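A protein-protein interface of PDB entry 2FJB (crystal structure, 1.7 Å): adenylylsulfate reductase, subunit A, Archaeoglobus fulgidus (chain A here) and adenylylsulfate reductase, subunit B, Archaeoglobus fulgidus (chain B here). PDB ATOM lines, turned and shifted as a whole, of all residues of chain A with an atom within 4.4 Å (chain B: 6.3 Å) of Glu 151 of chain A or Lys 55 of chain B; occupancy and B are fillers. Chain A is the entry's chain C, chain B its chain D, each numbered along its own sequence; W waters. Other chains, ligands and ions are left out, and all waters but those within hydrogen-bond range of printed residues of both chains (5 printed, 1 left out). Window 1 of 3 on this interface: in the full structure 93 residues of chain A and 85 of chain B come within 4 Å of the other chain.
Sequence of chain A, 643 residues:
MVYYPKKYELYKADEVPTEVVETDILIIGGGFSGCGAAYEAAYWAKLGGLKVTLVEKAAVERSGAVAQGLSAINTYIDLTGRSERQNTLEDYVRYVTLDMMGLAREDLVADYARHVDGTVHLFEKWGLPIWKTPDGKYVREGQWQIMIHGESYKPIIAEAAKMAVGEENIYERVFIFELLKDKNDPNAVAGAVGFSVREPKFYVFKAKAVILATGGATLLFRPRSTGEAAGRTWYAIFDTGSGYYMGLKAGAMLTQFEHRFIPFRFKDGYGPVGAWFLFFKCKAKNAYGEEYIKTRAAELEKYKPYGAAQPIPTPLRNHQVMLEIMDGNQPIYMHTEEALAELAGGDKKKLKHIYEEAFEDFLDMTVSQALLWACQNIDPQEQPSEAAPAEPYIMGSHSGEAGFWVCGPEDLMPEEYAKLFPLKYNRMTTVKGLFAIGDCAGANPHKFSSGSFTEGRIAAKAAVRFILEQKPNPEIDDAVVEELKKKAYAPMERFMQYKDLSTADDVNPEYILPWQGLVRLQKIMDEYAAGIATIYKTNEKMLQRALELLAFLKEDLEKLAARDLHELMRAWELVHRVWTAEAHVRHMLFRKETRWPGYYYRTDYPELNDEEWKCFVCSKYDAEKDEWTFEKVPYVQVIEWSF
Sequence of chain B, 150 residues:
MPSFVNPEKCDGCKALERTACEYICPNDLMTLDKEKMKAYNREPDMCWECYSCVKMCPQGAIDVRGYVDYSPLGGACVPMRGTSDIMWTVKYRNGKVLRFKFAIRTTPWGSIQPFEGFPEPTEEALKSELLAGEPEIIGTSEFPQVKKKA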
ATOM      1  N   ARG A  62     -19.092  13.678  -4.832  1.00  0.00           N
ATOM      2  CA  ARG A  62     -19.434  14.810  -3.965  1.00  0.00           C
ATOM      3  C   ARG A  62     -18.359  15.889  -3.873  1.00  0.00           C
ATOM      4  O   ARG A  62     -18.498  16.827  -3.094  1.00  0.00           O
ATOM      5  CB  ARG A  62     -19.715  14.308  -2.543  1.00  0.00           C
ATOM      6  CG  ARG A  62     -21.016  13.544  -2.370  1.00  0.00           C
ATOM      7  CD  ARG A  62     -22.207  14.491  -2.291  1.00  0.00           C
ATOM      8  NE  ARG A  62     -23.462  13.747  -2.232  1.00  0.00           N
ATOM      9  CZ  ARG A  62     -24.660  14.294  -2.067  1.00  0.00           C
ATOM     10  NH1 ARG A  62     -24.788  15.609  -1.931  1.00  0.00           N
ATOM     11  NH2 ARG A  62     -25.740  13.519  -2.067  1.00  0.00           N
ATOM     12  N   GLN A  68     -22.731  19.725  -0.855  1.00  0.00           N
ATOM     13  CA  GLN A  68     -23.987  19.660  -0.109  1.00  0.00           C
ATOM     14  C   GLN A  68     -25.196  19.747  -1.022  1.00  0.00           C
ATOM     15  O   GLN A  68     -26.318  19.437  -0.614  1.00  0.00           O
ATOM     16  CB  GLN A  68     -24.078  20.805   0.903  1.00  0.00           C
ATOM     17  CG  GLN A  68     -22.784  21.139   1.616  1.00  0.00           C
ATOM     18  CD  GLN A  68     -23.003  22.060   2.803  1.00  0.00           C
ATOM     19  OE1 GLN A  68     -22.125  22.850   3.164  1.00  0.00           O
ATOM     20  NE2 GLN A  68     -24.171  21.951   3.425  1.00  0.00           N
ATOM     21  N   GLY A  69     -24.948  20.159  -2.260  1.00  0.00           N
ATOM     22  CA  GLY A  69     -26.009  20.357  -3.225  1.00  0.00           C
ATOM     23  C   GLY A  69     -26.145  21.867  -3.330  1.00  0.00           C
ATOM     24  O   GLY A  69     -25.367  22.591  -2.713  1.00  0.00           O
ATOM     25  N   HIS A 149     -34.329  21.475  -6.641  1.00  0.00           N
ATOM     26  CA  HIS A 149     -34.304  20.583  -5.489  1.00  0.00           C
ATOM     27  C   HIS A 149     -32.958  19.924  -5.770  1.00  0.00           C
ATOM     28  O   HIS A 149     -32.890  18.807  -6.285  1.00  0.00           O
ATOM     29  CB  HIS A 149     -35.451  19.571  -5.574  1.00  0.00           C
ATOM     30  CG  HIS A 149     -36.811  20.191  -5.474  1.00  0.00           C
ATOM     31  ND1 HIS A 149     -37.254  20.833  -4.336  1.00  0.00           N
ATOM     32  CD2 HIS A 149     -37.825  20.270  -6.368  1.00  0.00           C
ATOM     33  CE1 HIS A 149     -38.482  21.280  -4.535  1.00  0.00           C
ATOM     34  NE2 HIS A 149     -38.852  20.951  -5.759  1.00  0.00           N
ATOM     35  N   GLY A 150     -31.886  20.642  -5.442  1.00  0.00           N
ATOM     36  CA  GLY A 150     -30.550  20.167  -5.757  1.00  0.00           C
ATOM     37  C   GLY A 150     -29.652  19.445  -4.776  1.00  0.00           C
ATOM     38  O   GLY A 150     -28.433  19.557  -4.886  1.00  0.00           O
ATOM     39  N   GLU A 151     -30.218  18.685  -3.846  1.00  0.00           N
ATOM     40  CA  GLU A 151     -29.393  17.963  -2.888  1.00  0.00           C
ATOM     41  C   GLU A 151     -28.395  17.043  -3.592  1.00  0.00           C
ATOM     42  O   GLU A 151     -27.245  16.927  -3.167  1.00  0.00           O
ATOM     43  CB  GLU A 151     -30.271  17.134  -1.942  1.00  0.00           C
ATOM     44  CG  GLU A 151     -29.490  16.437  -0.823  1.00  0.00           C
ATOM     45  CD  GLU A 151     -28.850  15.127  -1.260  1.00  0.00           C
ATOM     46  OE1 GLU A 151     -27.799  14.755  -0.691  1.00  0.00           O
ATOM     47  OE2 GLU A 151     -29.401  14.460  -2.161  1.00  0.00           O
ATOM     48  N   SER A 152     -28.837  16.394  -4.669  1.00  0.00           N
ATOM     49  CA  SER A 152     -27.986  15.468  -5.417  1.00  0.00           C
ATOM     50  C   SER A 152     -27.429  16.059  -6.701  1.00  0.00           C
ATOM     51  O   SER A 152     -27.074  15.328  -7.625  1.00  0.00           O
ATOM     52  CB  SER A 152     -28.763  14.188  -5.753  1.00  0.00           C
ATOM     53  OG  SER A 152     -29.049  13.444  -4.583  1.00  0.00           O
ATOM     54  N   TYR A 153     -27.344  17.383  -6.747  1.00  0.00           N
ATOM     55  CA  TYR A 153     -26.838  18.098  -7.911  1.00  0.00           C
ATOM     56  C   TYR A 153     -25.461  17.592  -8.367  1.00  0.00           C
ATOM     57  O   TYR A 153     -25.265  17.313  -9.551  1.00  0.00           O
ATOM     58  CB  TYR A 153     -26.791  19.595  -7.575  1.00  0.00           C
ATOM     59  CG  TYR A 153     -26.658  20.556  -8.738  1.00  0.00           C
ATOM     60  CD1 TYR A 153     -26.799  20.137 -10.066  1.00  0.00           C
ATOM     61  CD2 TYR A 153     -26.425  21.911  -8.496  1.00  0.00           C
ATOM     62  CE1 TYR A 153     -26.708  21.052 -11.121  1.00  0.00           C
ATOM     63  CE2 TYR A 153     -26.338  22.825  -9.536  1.00  0.00           C
ATOM     64  CZ  TYR A 153     -26.479  22.396 -10.842  1.00  0.00           C
ATOM     65  OH  TYR A 153     -26.383  23.325 -11.856  1.00  0.00           O
ATOM     66  N   ASP A 364     -30.570  22.068   1.378  1.00  0.00           N
ATOM     67  CA  ASP A 364     -30.123  21.623   0.058  1.00  0.00           C
ATOM     68  C   ASP A 364     -28.777  22.253  -0.288  1.00  0.00           C
ATOM     69  O   ASP A 364     -28.263  22.022  -1.381  1.00  0.00           O
ATOM     70  CB  ASP A 364     -31.084  22.099  -1.043  1.00  0.00           C
ATOM     71  CG  ASP A 364     -32.282  21.190  -1.255  1.00  0.00           C
ATOM     72  OD1 ASP A 364     -33.080  21.522  -2.158  1.00  0.00           O
ATOM     73  OD2 ASP A 364     -32.436  20.168  -0.554  1.00  0.00           O
ATOM     74  N   CYS B  50     -20.629  19.308   5.350  1.00  0.00           N
ATOM     75  CA  CYS B  50     -21.367  19.123   4.106  1.00  0.00           C
ATOM     76  C   CYS B  50     -22.350  17.956   4.200  1.00  0.00           C
ATOM     77  O   CYS B  50     -23.206  17.790   3.333  1.00  0.00           O
ATOM     78  CB  CYS B  50     -20.402  18.889   2.939  1.00  0.00           C
ATOM     79  SG  CYS B  50     -19.608  17.257   2.892  1.00  0.00           S
ATOM     80  N   TYR B  51     -22.209  17.156   5.256  1.00  0.00           N
ATOM     81  CA  TYR B  51     -23.071  16.000   5.510  1.00  0.00           C
ATOM     82  C   TYR B  51     -22.990  14.859   4.499  1.00  0.00           C
ATOM     83  O   TYR B  51     -23.858  13.988   4.491  1.00  0.00           O
ATOM     84  CB  TYR B  51     -24.538  16.434   5.633  1.00  0.00           C
ATOM     85  CG  TYR B  51     -24.911  17.025   6.976  1.00  0.00           C
ATOM     86  CD1 TYR B  51     -24.441  18.278   7.366  1.00  0.00           C
ATOM     87  CD2 TYR B  51     -25.734  16.327   7.860  1.00  0.00           C
ATOM     88  CE1 TYR B  51     -24.783  18.824   8.603  1.00  0.00           C
ATOM     89  CE2 TYR B  51     -26.085  16.866   9.103  1.00  0.00           C
ATOM     90  CZ  TYR B  51     -25.606  18.115   9.465  1.00  0.00           C
ATOM     91  OH  TYR B  51     -25.962  18.664  10.677  1.00  0.00           O
ATOM     92  N   SER B  52     -21.964  14.846   3.654  1.00  0.00           N
ATOM     93  CA  SER B  52     -21.838  13.773   2.667  1.00  0.00           C
ATOM     94  C   SER B  52     -21.641  12.424   3.356  1.00  0.00           C
ATOM     95  O   SER B  52     -22.280  11.435   2.995  1.00  0.00           O
ATOM     96  CB  SER B  52     -20.670  14.046   1.713  1.00  0.00           C
ATOM     97  OG  SER B  52     -20.954  15.147   0.856  1.00  0.00           O
ATOM     98  N   CYS B  53     -20.759  12.392   4.350  1.00  0.00           N
ATOM     99  CA  CYS B  53     -20.487  11.164   5.095  1.00  0.00           C
ATOM    100  C   CYS B  53     -21.746  10.692   5.825  1.00  0.00           C
ATOM    101  O   CYS B  53     -22.054   9.501   5.843  1.00  0.00           O
ATOM    102  CB  CYS B  53     -19.361  11.400   6.107  1.00  0.00           C
ATOM    103  SG  CYS B  53     -19.673  12.751   7.275  1.00  0.00           S
ATOM    104  N   VAL B  54     -22.464  11.638   6.425  1.00  0.00           N
ATOM    105  CA  VAL B  54     -23.693  11.345   7.157  1.00  0.00           C
ATOM    106  C   VAL B  54     -24.728  10.677   6.253  1.00  0.00           C
ATOM    107  O   VAL B  54     -25.338   9.673   6.624  1.00  0.00           O
ATOM    108  CB  VAL B  54     -24.310  12.641   7.745  1.00  0.00           C
ATOM    109  CG1 VAL B  54     -25.684  12.351   8.355  1.00  0.00           C
ATOM    110  CG2 VAL B  54     -23.383  13.223   8.801  1.00  0.00           C
ATOM    111  N   LYS B  55     -24.919  11.238   5.063  1.00  0.00           N
ATOM    112  CA  LYS B  55     -25.884  10.705   4.109  1.00  0.00           C
ATOM    113  C   LYS B  55     -25.511   9.344   3.527  1.00  0.00           C
ATOM    114  O   LYS B  55     -26.390   8.539   3.218  1.00  0.00           O
ATOM    115  CB  LYS B  55     -26.073  11.685   2.946  1.00  0.00           C
ATOM    116  CG  LYS B  55     -26.609  13.056   3.330  1.00  0.00           C
ATOM    117  CD  LYS B  55     -26.480  14.017   2.156  1.00  0.00           C
ATOM    118  CE  LYS B  55     -27.041  15.386   2.492  1.00  0.00           C
ATOM    119  NZ  LYS B  55     -26.779  16.342   1.379  1.00  0.00           N
ATOM    120  N   MET B  56     -24.215   9.091   3.369  1.00  0.00           N
ATOM    121  CA  MET B  56     -23.773   7.842   2.766  1.00  0.00           C
ATOM    122  C   MET B  56     -23.463   6.696   3.717  1.00  0.00           C
ATOM    123  O   MET B  56     -23.197   5.580   3.267  1.00  0.00           O
ATOM    124  CB  MET B  56     -22.568   8.102   1.856  1.00  0.00           C
ATOM    125  CG  MET B  56     -22.820   9.162   0.785  1.00  0.00           C
ATOM    126  SD  MET B  56     -24.453   9.042   0.004  1.00  0.00           S
ATOM    127  CE  MET B  56     -24.218   7.634  -1.097  1.00  0.00           C
ATOM    128  N   CYS B  57     -23.493   6.953   5.021  1.00  0.00           N
ATOM    129  CA  CYS B  57     -23.232   5.881   5.975  1.00  0.00           C
ATOM    130  C   CYS B  57     -24.459   4.982   6.013  1.00  0.00           C
ATOM    131  O   CYS B  57     -25.528   5.396   6.463  1.00  0.00           O
ATOM    132  CB  CYS B  57     -22.975   6.427   7.376  1.00  0.00           C
ATOM    133  SG  CYS B  57     -22.838   5.094   8.601  1.00  0.00           S
ATOM    134  N   PRO B  58     -24.317   3.734   5.539  1.00  0.00           N
ATOM    135  CA  PRO B  58     -25.422   2.771   5.515  1.00  0.00           C
ATOM    136  C   PRO B  58     -25.944   2.379   6.897  1.00  0.00           C
ATOM    137  O   PRO B  58     -27.048   1.844   7.020  1.00  0.00           O
ATOM    138  CB  PRO B  58     -24.827   1.588   4.754  1.00  0.00           C
ATOM    139  CG  PRO B  58     -23.383   1.641   5.140  1.00  0.00           C
ATOM    140  CD  PRO B  58     -23.073   3.118   5.044  1.00  0.00           C
ATOM    141  N   ILE B  62     -23.159   8.141  11.569  1.00  0.00           N
ATOM    142  CA  ILE B  62     -22.529   9.451  11.608  1.00  0.00           C
ATOM    143  C   ILE B  62     -23.541  10.573  11.790  1.00  0.00           C
ATOM    144  O   ILE B  62     -24.616  10.562  11.195  1.00  0.00           O
ATOM    145  CB  ILE B  62     -21.718   9.716  10.314  1.00  0.00           C
ATOM    146  CG1 ILE B  62     -20.803   8.523  10.013  1.00  0.00           C
ATOM    147  CG2 ILE B  62     -20.866  10.973  10.479  1.00  0.00           C
ATOM    148  CD1 ILE B  62     -19.968   8.692   8.744  1.00  0.00           C
ATOM    149  N   PRO B  79     -30.531  13.589   8.201  1.00  0.00           N
ATOM    150  CA  PRO B  79     -31.137  13.240   6.919  1.00  0.00           C
ATOM    151  C   PRO B  79     -31.311  11.734   6.745  1.00  0.00           C
ATOM    152  O   PRO B  79     -30.612  10.936   7.370  1.00  0.00           O
ATOM    153  CB  PRO B  79     -30.142  13.806   5.918  1.00  0.00           C
ATOM    154  CG  PRO B  79     -28.840  13.466   6.577  1.00  0.00           C
ATOM    155  CD  PRO B  79     -29.081  13.813   8.047  1.00  0.00           C
ATOM    156  N   ARG B  81     -31.623   9.890   3.333  1.00  0.00           N
ATOM    157  CA  ARG B  81     -31.600  10.016   1.884  1.00  0.00           C
ATOM    158  C   ARG B  81     -32.020   8.740   1.170  1.00  0.00           C
ATOM    159  O   ARG B  81     -31.494   7.661   1.440  1.00  0.00           O
ATOM    160  CB  ARG B  81     -30.194  10.437   1.447  1.00  0.00           C
ATOM    161  CG  ARG B  81     -30.030  10.740  -0.031  1.00  0.00           C
ATOM    162  CD  ARG B  81     -28.734  11.506  -0.260  1.00  0.00           C
ATOM    163  NE  ARG B  81     -28.436  11.692  -1.677  1.00  0.00           N
ATOM    164  CZ  ARG B  81     -27.890  10.765  -2.455  1.00  0.00           C
ATOM    165  NH1 ARG B  81     -27.574   9.575  -1.958  1.00  0.00           N
ATOM    166  NH2 ARG B  81     -27.660  11.025  -3.736  1.00  0.00           N
ATOM    167  N   ILE B  86     -35.319  12.982  -0.180  1.00  0.00           N
ATOM    168  CA  ILE B  86     -34.553  12.976   1.054  1.00  0.00           C
ATOM    169  C   ILE B  86     -35.428  13.525   2.168  1.00  0.00           C
ATOM    170  O   ILE B  86     -36.168  14.489   1.974  1.00  0.00           O
ATOM    171  CB  ILE B  86     -33.266  13.843   0.930  1.00  0.00           C
ATOM    172  CG1 ILE B  86     -32.464  13.776   2.233  1.00  0.00           C
ATOM    173  CG2 ILE B  86     -33.629  15.292   0.610  1.00  0.00           C
ATOM    174  CD1 ILE B  86     -31.100  14.442   2.148  1.00  0.00           C
ATOM    175  N   TRP B  88     -35.642  15.027   6.130  1.00  0.00           N
ATOM    176  CA  TRP B  88     -34.840  15.712   7.131  1.00  0.00           C
ATOM    177  C   TRP B  88     -35.636  15.915   8.404  1.00  0.00           C
ATOM    178  O   TRP B  88     -36.830  16.213   8.366  1.00  0.00           O
ATOM    179  CB  TRP B  88     -34.401  17.103   6.660  1.00  0.00           C
ATOM    180  CG  TRP B  88     -33.290  17.135   5.673  1.00  0.00           C
ATOM    181  CD1 TRP B  88     -33.403  17.208   4.316  1.00  0.00           C
ATOM    182  CD2 TRP B  88     -31.888  17.142   5.963  1.00  0.00           C
ATOM    183  NE1 TRP B  88     -32.156  17.266   3.739  1.00  0.00           N
ATOM    184  CE2 TRP B  88     -31.208  17.227   4.728  1.00  0.00           C
ATOM    185  CE3 TRP B  88     -31.138  17.086   7.147  1.00  0.00           C
ATOM    186  CZ2 TRP B  88     -29.813  17.260   4.639  1.00  0.00           C
ATOM    187  CZ3 TRP B  88     -29.749  17.120   7.060  1.00  0.00           C
ATOM    188  CH2 TRP B  88     -29.102  17.207   5.812  1.00  0.00           C
ATOM    189  N   ALA B 103     -37.550  16.386  -2.977  1.00  0.00           N
ATOM    190  CA  ALA B 103     -37.182  15.514  -4.084  1.00  0.00           C
ATOM    191  C   ALA B 103     -35.686  15.711  -4.344  1.00  0.00           C
ATOM    192  O   ALA B 103     -35.147  16.786  -4.071  1.00  0.00           O
ATOM    193  CB  ALA B 103     -37.983  15.886  -5.330  1.00  0.00           C
ATOM    194  N   ILE B 104     -35.011  14.678  -4.843  1.00  0.00           N
ATOM    195  CA  ILE B 104     -33.586  14.793  -5.154  1.00  0.00           C
ATOM    196  C   ILE B 104     -33.282  14.353  -6.585  1.00  0.00           C
ATOM    197  O   ILE B 104     -32.274  14.762  -7.165  1.00  0.00           O
ATOM    198  CB  ILE B 104     -32.686  13.987  -4.170  1.00  0.00           C
ATOM    199  CG1 ILE B 104     -32.951  12.485  -4.299  1.00  0.00           C
ATOM    200  CG2 ILE B 104     -32.925  14.462  -2.742  1.00  0.00           C
ATOM    201  CD1 ILE B 104     -32.047  11.632  -3.416  1.00  0.00           C
ATOM    202  N   TRP B 109     -31.285   6.107 -10.656  1.00  0.00           N
ATOM    203  CA  TRP B 109     -29.850   6.307 -10.539  1.00  0.00           C
ATOM    204  C   TRP B 109     -29.094   5.435 -11.531  1.00  0.00           C
ATOM    205  O   TRP B 109     -29.438   4.268 -11.742  1.00  0.00           O
ATOM    206  CB  TRP B 109     -29.385   6.028  -9.108  1.00  0.00           C
ATOM    207  CG  TRP B 109     -29.749   7.143  -8.195  1.00  0.00           C
ATOM    208  CD1 TRP B 109     -30.940   7.322  -7.549  1.00  0.00           C
ATOM    209  CD2 TRP B 109     -28.968   8.311  -7.928  1.00  0.00           C
ATOM    210  NE1 TRP B 109     -30.951   8.534  -6.902  1.00  0.00           N
ATOM    211  CE2 TRP B 109     -29.751   9.162  -7.117  1.00  0.00           C
ATOM    212  CE3 TRP B 109     -27.682   8.724  -8.298  1.00  0.00           C
ATOM    213  CZ2 TRP B 109     -29.291  10.405  -6.673  1.00  0.00           C
ATOM    214  CZ3 TRP B 109     -27.223   9.963  -7.856  1.00  0.00           C
ATOM    215  CH2 TRP B 109     -28.028  10.786  -7.053  1.00  0.00           C
HETATM  216  O   HOH W   1     -30.912  16.890  -6.603  1.00  0.00           O
HETATM  217  O   HOH W   2     -23.919  16.242   1.267  1.00  0.00           O
HETATM  218  O   HOH W   3     -24.017  10.979  -2.502  1.00  0.00           O
HETATM  219  O   HOH W   4     -31.451  18.407   1.206  1.00  0.00           O
HETATM  220  O   HOH W   5     -27.569  18.853   1.775  1.00  0.00           O
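NZ of Lys 55 of chain B is in salt-bridge range of OE1 of Glu 151 of chain A. The side-chain carboxylate of Glu 151 of chain A is in salt-bridge range of the guanidinium group of Arg 81 of chain B. The guanidinium group (NH2) of Arg 81 of chain B lies within hydrogen-bond range of the side-chain hydroxyl (OG) of Ser 152 of chain A, at 2.9 Å. NH2 of Arg 62 of chain A lies close to NE of Arg 81 of chain B (3.3 Å).
Hydrophobic or aromatic side chains of chain A that line the printed part of chain B: His 149. Along chain A the printed residues that touch a printed residue of chain B span positions 62 to 152. Hydrophobic or aromatic side chains of chain B within 4 Å of the printed part of chain A: Ile 86, Ile 104 and Trp 109. Among the printed residues, 13 pairs touch across the chains.
Water W1 lies within hydrogen-bond range of O of Ile 104 of chain B (2.6 Å), O of His 149 of chain A (2.8 Å), N of Ser 152 of chain A (2.9 Å) and N of Glu 151 of chain A (3.4 Å). Water W5 bridges NZ of Lys 55 of chain B (2.7 Å) and O of Gln 68 of chain A (2.8 Å). Water W4 lies within hydrogen-bond range of OD2 of Asp 364 of chain A and NE1 of Trp 88 of chain B. Water W2 lies within hydrogen-bond range of the backbone carbonyl oxygen of Cys 50 of chain B (2.7 Å), the side-chain amino group of Lys 55 of chain B (2.9 Å), the side-chain hydroxyl of Ser 52 of chain B (3.2 Å) and the guanidinium group of Arg 62 of chain A (3.4 Å). Water W3 bridges the guanidinium group (NE) of Arg 62 of chain A (2.8 Å) and the side-chain sulfur (SD) of Met 56 of chain B (3.2 Å).
The guanidinium group (NH2) of Arg 62 of chain A lies within salt-bridge range of the side-chain carboxylate (OE1) of Glu 151 of chain A, at 2.8 Å. The side-chain carboxylate (OE2) of Glu 151 of chain A lies within hydrogen-bond range of the side-chain hydroxyl (OG) of Ser 152 of chain A (2.6 Å). SG of Cys 50 of chain B lies close to OG of Ser 52 of chain B (3.2 Å). NH1 of Arg 81 of chain B lies within hydrogen-bond range of SD of Met 56 of chain B (3.7 Å).
Arg 62 of chain A touches Ser 52 of chain B. Arg 62 of chain A touches Lys 55 of chain B. CG of Gln 68 of chain A touches CA of Cys 50 of chain B (3.5 Å). Gln 68 of chain A touches Lys 55 of chain B (O to NZ, 3.7 Å). His 149 of chain A touches Ala 103 of chain B. Ile 86 of chain B touches Glu 151 of chain A (CD1 to CG, 3.9 Å). Ile 104 of chain B touches Glu 151 of chain A (CG2 to OE2, 3.6 Å). CD1 of Ile 104 of chain B touches OG of Ser 152 of chain A, 3.7 Å away. Trp 109 of chain B touches Ser 152 of chain A.
Of the printed residues of chain B, His 149 of chain A touches Ala 103. Of chain B, only Lys 55 (2.8 Å), Arg 81 (3.0 Å), Ile 86 (3.9 Å) and Ile 104 (3.6 Å) come within 4 Å of Glu 151 of chain A. Of the printed residues of chain B, Ser 152 of chain A touches Arg 81 (2.9 Å), Ile 104 (3.7 Å) and Trp 109 (3.7 Å). Of the printed residues of chain A, Lys 55 of chain B touches Arg 62, Gln 68 and Glu 151. Of the printed residues of chain A, Ile 104 of chain B touches Glu 151 and Ser 152. The nearest printed residue of chain A that does not touch Lys 55 of chain B is Gly 69 of chain A (5.6 Å).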
